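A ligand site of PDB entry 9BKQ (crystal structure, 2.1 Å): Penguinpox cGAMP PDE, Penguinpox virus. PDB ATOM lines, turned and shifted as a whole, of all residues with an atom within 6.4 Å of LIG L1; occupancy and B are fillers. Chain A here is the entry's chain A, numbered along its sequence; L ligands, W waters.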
ATOM      1  N   ARG A  17      -1.595  37.610   9.366  1.00  0.00           N
ATOM      2  CA  ARG A  17      -1.352  36.427  10.192  1.00  0.00           C
ATOM      3  C   ARG A  17      -1.442  36.761  11.674  1.00  0.00           C
ATOM      4  O   ARG A  17      -2.038  36.002  12.454  1.00  0.00           O
ATOM      5  CB  ARG A  17       0.017  35.831   9.872  1.00  0.00           C
ATOM      6  CG  ARG A  17       0.035  34.923   8.663  1.00  0.00           C
ATOM      7  CD  ARG A  17      -0.834  33.708   8.884  1.00  0.00           C
ATOM      8  NE  ARG A  17      -0.092  32.614   9.494  1.00  0.00           N
ATOM      9  CZ  ARG A  17      -0.306  31.330   9.240  1.00  0.00           C
ATOM     10  NH1 ARG A  17      -1.246  30.948   8.389  1.00  0.00           N
ATOM     11  NH2 ARG A  17       0.446  30.413   9.835  1.00  0.00           N
ATOM     12  N   ASP A  22      -9.135  32.446  15.761  1.00  0.00           N
ATOM     13  CA  ASP A  22     -10.360  31.708  15.467  1.00  0.00           C
ATOM     14  C   ASP A  22     -10.512  31.135  14.043  1.00  0.00           C
ATOM     15  O   ASP A  22     -11.502  31.318  13.388  1.00  0.00           O
ATOM     16  CB  ASP A  22     -11.576  32.557  15.947  1.00  0.00           C
ATOM     17  CG  ASP A  22     -12.859  31.886  15.829  1.00  0.00           C
ATOM     18  OD1 ASP A  22     -12.987  30.774  16.342  1.00  0.00           O
ATOM     19  OD2 ASP A  22     -13.763  32.494  15.256  1.00  0.00           O
ATOM     20  N   THR A  23      -9.472  30.511  13.554  1.00  0.00           N
ATOM     21  CA  THR A  23      -9.518  29.856  12.282  1.00  0.00           C
ATOM     22  C   THR A  23      -9.731  28.352  12.475  1.00  0.00           C
ATOM     23  O   THR A  23      -9.695  27.893  13.547  1.00  0.00           O
ATOM     24  CB  THR A  23      -8.225  30.097  11.511  1.00  0.00           C
ATOM     25  OG1 THR A  23      -7.166  29.943  12.393  1.00  0.00           O
ATOM     26  CG2 THR A  23      -8.129  31.474  11.053  1.00  0.00           C
ATOM     27  N   ILE A  24     -10.001  27.612  11.432  1.00  0.00           N
ATOM     28  CA  ILE A  24     -10.145  26.190  11.553  1.00  0.00           C
ATOM     29  C   ILE A  24      -9.029  25.410  10.893  1.00  0.00           C
ATOM     30  O   ILE A  24      -8.535  25.820   9.890  1.00  0.00           O
ATOM     31  CB  ILE A  24     -11.470  25.657  11.012  1.00  0.00           C
ATOM     32  CG1 ILE A  24     -11.634  26.007   9.555  1.00  0.00           C
ATOM     33  CG2 ILE A  24     -12.612  26.193  11.841  1.00  0.00           C
ATOM     34  CD1 ILE A  24     -12.928  25.559   8.967  1.00  0.00           C
ATOM     35  N   LEU A  25      -8.666  24.276  11.475  1.00  0.00           N
ATOM     36  CA  LEU A  25      -7.598  23.449  10.923  1.00  0.00           C
ATOM     37  C   LEU A  25      -8.192  22.355  10.057  1.00  0.00           C
ATOM     38  O   LEU A  25      -9.060  21.594  10.511  1.00  0.00           O
ATOM     39  CB  LEU A  25      -6.762  22.837  12.050  1.00  0.00           C
ATOM     40  CG  LEU A  25      -5.830  21.684  11.671  1.00  0.00           C
ATOM     41  CD1 LEU A  25      -4.748  22.138  10.719  1.00  0.00           C
ATOM     42  CD2 LEU A  25      -5.232  21.054  12.921  1.00  0.00           C
ATOM     43  N   ILE A  59      -2.901  33.091  15.953  1.00  0.00           N
ATOM     44  CA  ILE A  59      -2.476  31.788  15.448  1.00  0.00           C
ATOM     45  C   ILE A  59      -0.999  31.756  15.106  1.00  0.00           C
ATOM     46  O   ILE A  59      -0.445  30.676  14.866  1.00  0.00           O
ATOM     47  CB  ILE A  59      -3.308  31.378  14.215  1.00  0.00           C
ATOM     48  CG1 ILE A  59      -2.927  32.225  12.999  1.00  0.00           C
ATOM     49  CG2 ILE A  59      -4.806  31.483  14.520  1.00  0.00           C
ATOM     50  CD1 ILE A  59      -3.609  31.799  11.718  1.00  0.00           C
ATOM     51  N   ALA A  60      -0.330  32.908  15.069  1.00  0.00           N
ATOM     52  CA  ALA A  60       1.094  32.968  14.775  1.00  0.00           C
ATOM     53  C   ALA A  60       1.954  32.512  15.947  1.00  0.00           C
ATOM     54  O   ALA A  60       3.154  32.281  15.750  1.00  0.00           O
ATOM     55  CB  ALA A  60       1.490  34.380  14.360  1.00  0.00           C
ATOM     56  N   TYR A  63       0.040  28.230  18.746  1.00  0.00           N
ATOM     57  CA  TYR A  63       0.407  26.840  18.624  1.00  0.00           C
ATOM     58  C   TYR A  63       1.884  26.498  18.825  1.00  0.00           C
ATOM     59  O   TYR A  63       2.289  25.388  18.603  1.00  0.00           O
ATOM     60  CB  TYR A  63      -0.122  26.294  17.310  1.00  0.00           C
ATOM     61  CG  TYR A  63      -1.573  26.490  17.211  1.00  0.00           C
ATOM     62  CD1 TYR A  63      -2.432  25.648  17.841  1.00  0.00           C
ATOM     63  CD2 TYR A  63      -2.081  27.574  16.568  1.00  0.00           C
ATOM     64  CE1 TYR A  63      -3.768  25.844  17.805  1.00  0.00           C
ATOM     65  CE2 TYR A  63      -3.433  27.778  16.518  1.00  0.00           C
ATOM     66  CZ  TYR A  63      -4.258  26.895  17.139  1.00  0.00           C
ATOM     67  OH  TYR A  63      -5.558  27.096  17.100  1.00  0.00           O
ATOM     68  N   ILE A  69       2.510  18.744  20.907  1.00  0.00           N
ATOM     69  CA  ILE A  69       1.795  18.949  19.645  1.00  0.00           C
ATOM     70  C   ILE A  69       1.118  17.656  19.225  1.00  0.00           C
ATOM     71  O   ILE A  69       1.777  16.605  19.172  1.00  0.00           O
ATOM     72  CB  ILE A  69       2.738  19.458  18.545  1.00  0.00           C
ATOM     73  CG1 ILE A  69       3.540  20.655  19.032  1.00  0.00           C
ATOM     74  CG2 ILE A  69       1.944  19.815  17.285  1.00  0.00           C
ATOM     75  CD1 ILE A  69       4.612  21.112  18.057  1.00  0.00           C
ATOM     76  N   HIS A  72       0.067  15.609  13.358  1.00  0.00           N
ATOM     77  CA  HIS A  72      -0.872  15.910  12.288  1.00  0.00           C
ATOM     78  C   HIS A  72      -0.116  16.490  11.092  1.00  0.00           C
ATOM     79  O   HIS A  72       0.974  17.045  11.242  1.00  0.00           O
ATOM     80  CB  HIS A  72      -1.943  16.909  12.754  1.00  0.00           C
ATOM     81  CG  HIS A  72      -1.405  18.271  13.059  1.00  0.00           C
ATOM     82  ND1 HIS A  72      -0.810  18.587  14.256  1.00  0.00           N
ATOM     83  CD2 HIS A  72      -1.373  19.399  12.316  1.00  0.00           C
ATOM     84  CE1 HIS A  72      -0.429  19.850  14.243  1.00  0.00           C
ATOM     85  NE2 HIS A  72      -0.765  20.369  13.069  1.00  0.00           N
ATOM     86  N   VAL A  73      -0.727  16.352   9.926  1.00  0.00           N
ATOM     87  CA  VAL A  73      -0.249  16.964   8.695  1.00  0.00           C
ATOM     88  C   VAL A  73      -1.308  17.971   8.253  1.00  0.00           C
ATOM     89  O   VAL A  73      -2.419  17.586   7.874  1.00  0.00           O
ATOM     90  CB  VAL A  73       0.027  15.934   7.591  1.00  0.00           C
ATOM     91  CG1 VAL A  73       0.403  16.642   6.296  1.00  0.00           C
ATOM     92  CG2 VAL A  73       1.130  14.974   8.027  1.00  0.00           C
ATOM     93  N   THR A  74      -0.958  19.260   8.323  1.00  0.00           N
ATOM     94  CA  THR A  74      -1.897  20.305   7.930  1.00  0.00           C
ATOM     95  C   THR A  74      -2.089  20.309   6.416  1.00  0.00           C
ATOM     96  O   THR A  74      -1.110  20.315   5.666  1.00  0.00           O
ATOM     97  CB  THR A  74      -1.387  21.671   8.396  1.00  0.00           C
ATOM     98  OG1 THR A  74      -1.294  21.695   9.816  1.00  0.00           O
ATOM     99  CG2 THR A  74      -2.335  22.773   7.929  1.00  0.00           C
ATOM    100  N   ILE A  77      -5.355  25.960   6.469  1.00  0.00           N
ATOM    101  CA  ILE A  77      -5.994  26.712   7.530  1.00  0.00           C
ATOM    102  C   ILE A  77      -6.880  27.770   6.892  1.00  0.00           C
ATOM    103  O   ILE A  77      -6.438  28.470   5.972  1.00  0.00           O
ATOM    104  CB  ILE A  77      -4.969  27.362   8.476  1.00  0.00           C
ATOM    105  CG1 ILE A  77      -3.989  26.317   9.015  1.00  0.00           C
ATOM    106  CG2 ILE A  77      -5.668  28.070   9.623  1.00  0.00           C
ATOM    107  CD1 ILE A  77      -4.623  25.277   9.894  1.00  0.00           C
ATOM    108  N   THR A  78      -8.121  27.885   7.352  1.00  0.00           N
ATOM    109  CA  THR A  78      -9.056  28.841   6.797  1.00  0.00           C
ATOM    110  C   THR A  78      -9.901  29.427   7.919  1.00  0.00           C
ATOM    111  O   THR A  78      -9.723  29.103   9.098  1.00  0.00           O
ATOM    112  CB  THR A  78      -9.938  28.194   5.712  1.00  0.00           C
ATOM    113  OG1 THR A  78     -10.661  29.205   5.011  1.00  0.00           O
ATOM    114  CG2 THR A  78     -10.925  27.218   6.347  1.00  0.00           C
ATOM    115  N   PHE A 111      12.232  25.125  10.093  1.00  0.00           N
ATOM    116  CA  PHE A 111      11.694  26.261   9.353  1.00  0.00           C
ATOM    117  C   PHE A 111      12.314  27.559   9.848  1.00  0.00           C
ATOM    118  O   PHE A 111      12.720  27.667  11.009  1.00  0.00           O
ATOM    119  CB  PHE A 111      10.175  26.346   9.523  1.00  0.00           C
ATOM    120  CG  PHE A 111       9.403  25.332   8.719  1.00  0.00           C
ATOM    121  CD1 PHE A 111       9.962  24.741   7.602  1.00  0.00           C
ATOM    122  CD2 PHE A 111       8.118  24.987   9.077  1.00  0.00           C
ATOM    123  CE1 PHE A 111       9.256  23.811   6.866  1.00  0.00           C
ATOM    124  CE2 PHE A 111       7.398  24.060   8.343  1.00  0.00           C
ATOM    125  CZ  PHE A 111       7.974  23.471   7.237  1.00  0.00           C
ATOM    126  N   ALA A 126      10.380  26.171  14.376  1.00  0.00           N
ATOM    127  CA  ALA A 126       9.766  24.847  14.301  1.00  0.00           C
ATOM    128  C   ALA A 126      10.718  23.861  13.644  1.00  0.00           C
ATOM    129  O   ALA A 126      11.229  24.112  12.549  1.00  0.00           O
ATOM    130  CB  ALA A 126       8.458  24.909  13.517  1.00  0.00           C
ATOM    131  N   VAL A 128      10.639  20.310  11.978  1.00  0.00           N
ATOM    132  CA  VAL A 128       9.604  19.485  11.372  1.00  0.00           C
ATOM    133  C   VAL A 128      10.260  18.359  10.572  1.00  0.00           C
ATOM    134  O   VAL A 128      11.411  18.448  10.159  1.00  0.00           O
ATOM    135  CB  VAL A 128       8.670  20.295  10.460  1.00  0.00           C
ATOM    136  CG1 VAL A 128       8.285  21.616  11.126  1.00  0.00           C
ATOM    137  CG2 VAL A 128       9.314  20.537   9.093  1.00  0.00           C
ATOM    138  N   HIS A 167       4.426  18.275   6.098  1.00  0.00           N
ATOM    139  CA  HIS A 167       5.328  18.041   7.214  1.00  0.00           C
ATOM    140  C   HIS A 167       4.526  17.702   8.455  1.00  0.00           C
ATOM    141  O   HIS A 167       3.340  18.039   8.570  1.00  0.00           O
ATOM    142  CB  HIS A 167       6.201  19.270   7.484  1.00  0.00           C
ATOM    143  CG  HIS A 167       5.430  20.466   7.938  1.00  0.00           C
ATOM    144  ND1 HIS A 167       4.822  21.336   7.059  1.00  0.00           N
ATOM    145  CD2 HIS A 167       5.147  20.925   9.189  1.00  0.00           C
ATOM    146  CE1 HIS A 167       4.212  22.289   7.742  1.00  0.00           C
ATOM    147  NE2 HIS A 167       4.393  22.064   9.031  1.00  0.00           N
ATOM    148  N   VAL A 168       5.187  17.019   9.382  1.00  0.00           N
ATOM    149  CA  VAL A 168       4.689  16.818  10.735  1.00  0.00           C
ATOM    150  C   VAL A 168       5.642  17.567  11.662  1.00  0.00           C
ATOM    151  O   VAL A 168       6.815  17.199  11.788  1.00  0.00           O
ATOM    152  CB  VAL A 168       4.626  15.324  11.103  1.00  0.00           C
ATOM    153  CG1 VAL A 168       3.833  15.135  12.395  1.00  0.00           C
ATOM    154  CG2 VAL A 168       4.007  14.535   9.966  1.00  0.00           C
ATOM    155  N   THR A 169       5.133  18.628  12.294  1.00  0.00           N
ATOM    156  CA  THR A 169       5.957  19.391  13.218  1.00  0.00           C
ATOM    157  C   THR A 169       6.253  18.568  14.462  1.00  0.00           C
ATOM    158  O   THR A 169       5.349  17.978  15.055  1.00  0.00           O
ATOM    159  CB  THR A 169       5.254  20.700  13.597  1.00  0.00           C
ATOM    160  OG1 THR A 169       5.057  21.481  12.413  1.00  0.00           O
ATOM    161  CG2 THR A 169       6.095  21.487  14.585  1.00  0.00           C
ATOM    162  N   TYR A 172       9.032  22.983  18.779  1.00  0.00           N
ATOM    163  CA  TYR A 172       9.610  24.313  18.644  1.00  0.00           C
ATOM    164  C   TYR A 172      10.755  24.463  19.630  1.00  0.00           C
ATOM    165  O   TYR A 172      10.666  24.033  20.786  1.00  0.00           O
ATOM    166  CB  TYR A 172       8.559  25.401  18.883  1.00  0.00           C
ATOM    167  CG  TYR A 172       7.391  25.365  17.929  1.00  0.00           C
ATOM    168  CD1 TYR A 172       6.306  24.528  18.156  1.00  0.00           C
ATOM    169  CD2 TYR A 172       7.369  26.169  16.801  1.00  0.00           C
ATOM    170  CE1 TYR A 172       5.235  24.495  17.293  1.00  0.00           C
ATOM    171  CE2 TYR A 172       6.296  26.140  15.921  1.00  0.00           C
ATOM    172  CZ  TYR A 172       5.231  25.301  16.175  1.00  0.00           C
ATOM    173  OH  TYR A 172       4.160  25.267  15.312  1.00  0.00           O
HETATM  174  C1  LIG L   1       0.434  26.945  12.658  1.00  0.00           C
HETATM  175  C2  LIG L   1      -0.469  25.777  12.637  1.00  0.00           C
HETATM  176  C3  LIG L   1      -0.096  24.635  12.109  1.00  0.00           C
HETATM  177  C4  LIG L   1      -1.444  24.115  12.393  1.00  0.00           C
HETATM  178  C5  LIG L   1      -1.701  24.463  13.912  1.00  0.00           C
HETATM  179  C6  LIG L   1      -3.800  23.836  14.980  1.00  0.00           C
HETATM  180  C7  LIG L   1      -5.057  25.359  14.410  1.00  0.00           C
HETATM  181  C8  LIG L   1      -6.056  26.269  14.121  1.00  0.00           C
HETATM  182  C9  LIG L   1      -4.598  27.495  12.937  1.00  0.00           C
HETATM  183  C10 LIG L   1      -3.828  25.621  13.912  1.00  0.00           C
HETATM  184  N1  LIG L   1      -3.059  24.667  14.315  1.00  0.00           N
HETATM  185  N2  LIG L   1      -4.997  24.243  15.079  1.00  0.00           N
HETATM  186  N3  LIG L   1      -7.375  26.044  14.605  1.00  0.00           N
HETATM  187  N4  LIG L   1      -5.794  27.314  13.405  1.00  0.00           N
HETATM  188  N5  LIG L   1      -3.628  26.667  13.179  1.00  0.00           N
HETATM  189  O1  LIG L   1      -0.473  27.882  12.196  1.00  0.00           O
HETATM  190  O2  LIG L   1       0.813  23.815  12.698  1.00  0.00           O
HETATM  191  O3  LIG L   1       1.310  22.075  10.879  1.00  0.00           O
HETATM  192  O4  LIG L   1       2.526  22.038  12.788  1.00  0.00           O
HETATM  193  O5  LIG L   1      -1.546  22.810  12.094  1.00  0.00           O
HETATM  194  O6  LIG L   1      -1.195  25.610  14.027  1.00  0.00           O
HETATM  195  P1  LIG L   1       1.891  22.932  11.853  1.00  0.00           P
HETATM  196  S1  LIG L   1       3.464  24.147  11.157  1.00  0.00           S
HETATM  197  N1  LG2 L   2       6.574  27.226   6.656  1.00  0.00           N
HETATM  198  C1  LG2 L   2       7.690  28.003   6.505  1.00  0.00           C
HETATM  199  N2  LG2 L   2       8.152  27.964   5.299  1.00  0.00           N
HETATM  200  C2  LG2 L   2       7.319  27.116   4.619  1.00  0.00           C
HETATM  201  C3  LG2 L   2       7.322  26.671   3.263  1.00  0.00           C
HETATM  202  O1  LG2 L   2       8.096  26.958   2.367  1.00  0.00           O
HETATM  203  N3  LG2 L   2       6.253  25.799   3.010  1.00  0.00           N
HETATM  204  C4  LG2 L   2       5.319  25.387   3.924  1.00  0.00           C
HETATM  205  N4  LG2 L   2       4.369  24.546   3.489  1.00  0.00           N
HETATM  206  N5  LG2 L   2       5.318  25.797   5.168  1.00  0.00           N
HETATM  207  C5  LG2 L   2       6.316  26.642   5.466  1.00  0.00           C
HETATM  208  O   HOH W   1      -0.121  22.623  16.096  1.00  0.00           O
HETATM  209  O   HOH W   2      -0.208  27.250   8.893  1.00  0.00           O
HETATM  210  O   HOH W   3       1.636  20.404   9.017  1.00  0.00           O
HETATM  211  O   HOH W   4      -7.365  22.924  15.994  1.00  0.00           O
HETATM  212  O   HOH W   5       2.550  22.700  15.268  1.00  0.00           O
HETATM  213  O   HOH W   6       1.159  24.423   8.994  1.00  0.00           O
HETATM  214  O   HOH W   7       2.440  19.386  11.991  1.00  0.00           O
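NH2 of Arg 17 touches O1 of LIG L1 (3.6 Å).
Leu 25 touches LIG L1 (CD1 to O5, 3.5 Å).
Ile 59 touches LIG L1.
Ile 77 touches LIG L1 (CG2 to C9, 3.5 Å).
Of the 21 residues printed, 10 come within 4 Å of LIG L1.
Along chain A the residues within 4 Å of LIG L1 span positions 17 to 169.
The nearest printed residue that does not touch LIG L1 is Ile 24 (4.1 Å).
The side-chain hydroxyl of Thr 169 sits close to a ring nitrogen (NE2) of His 167 (3.5 Å).
An oxygen (O5) of LIG L1 lies within hydrogen-bond range of the side-chain hydroxyl (OG1) of Thr 74, 2.5 Å away.
OG1 of Thr 169 sits at hydrogen-bond distance from O4 of LIG L1, 2.6 Å away.
A ring nitrogen (NE2) of His 72 lies within hydrogen-bond range of an oxygen (O5) of LIG L1, 2.7 Å away.
A ring nitrogen (NE2) of His 167 lies close to a sulfur (S1) of LIG L1 (3.1 Å).
A nitrogen (N3) of LIG L1 sits close to the side-chain hydroxyl (OH) of Tyr 63 (3.3 Å).
N3 of LIG L1 lies within hydrogen-bond range of O of Thr 23 (3.1 Å).
The side-chain hydroxyl (OG1) of Thr 23 sits at hydrogen-bond distance from a nitrogen (N4) of LIG L1 (3.1 Å).
Water W3 lies within hydrogen-bond range of an oxygen (O3) of LIG L1 (2.5 Å), the backbone NH of Thr 74 (2.9 Å) and the backbone carbonyl oxygen of His 167 (2.9 Å).
Water W5 bridges an oxygen (O4) of LIG L1 (2.6 Å) and the side-chain hydroxyl (OH) of Tyr 172 (3.0 Å).
Water W7 lies within hydrogen-bond range of an oxygen (O4) of LIG L1 (2.8 Å), the backbone NH of Thr 169 (2.8 Å) and the backbone carbonyl oxygen of His 72 (2.9 Å).
Water W2 bridges the guanidinium group (NH2) of Arg 17 (3.4 Å) and an oxygen (O1) of LIG L1 (3.4 Å).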
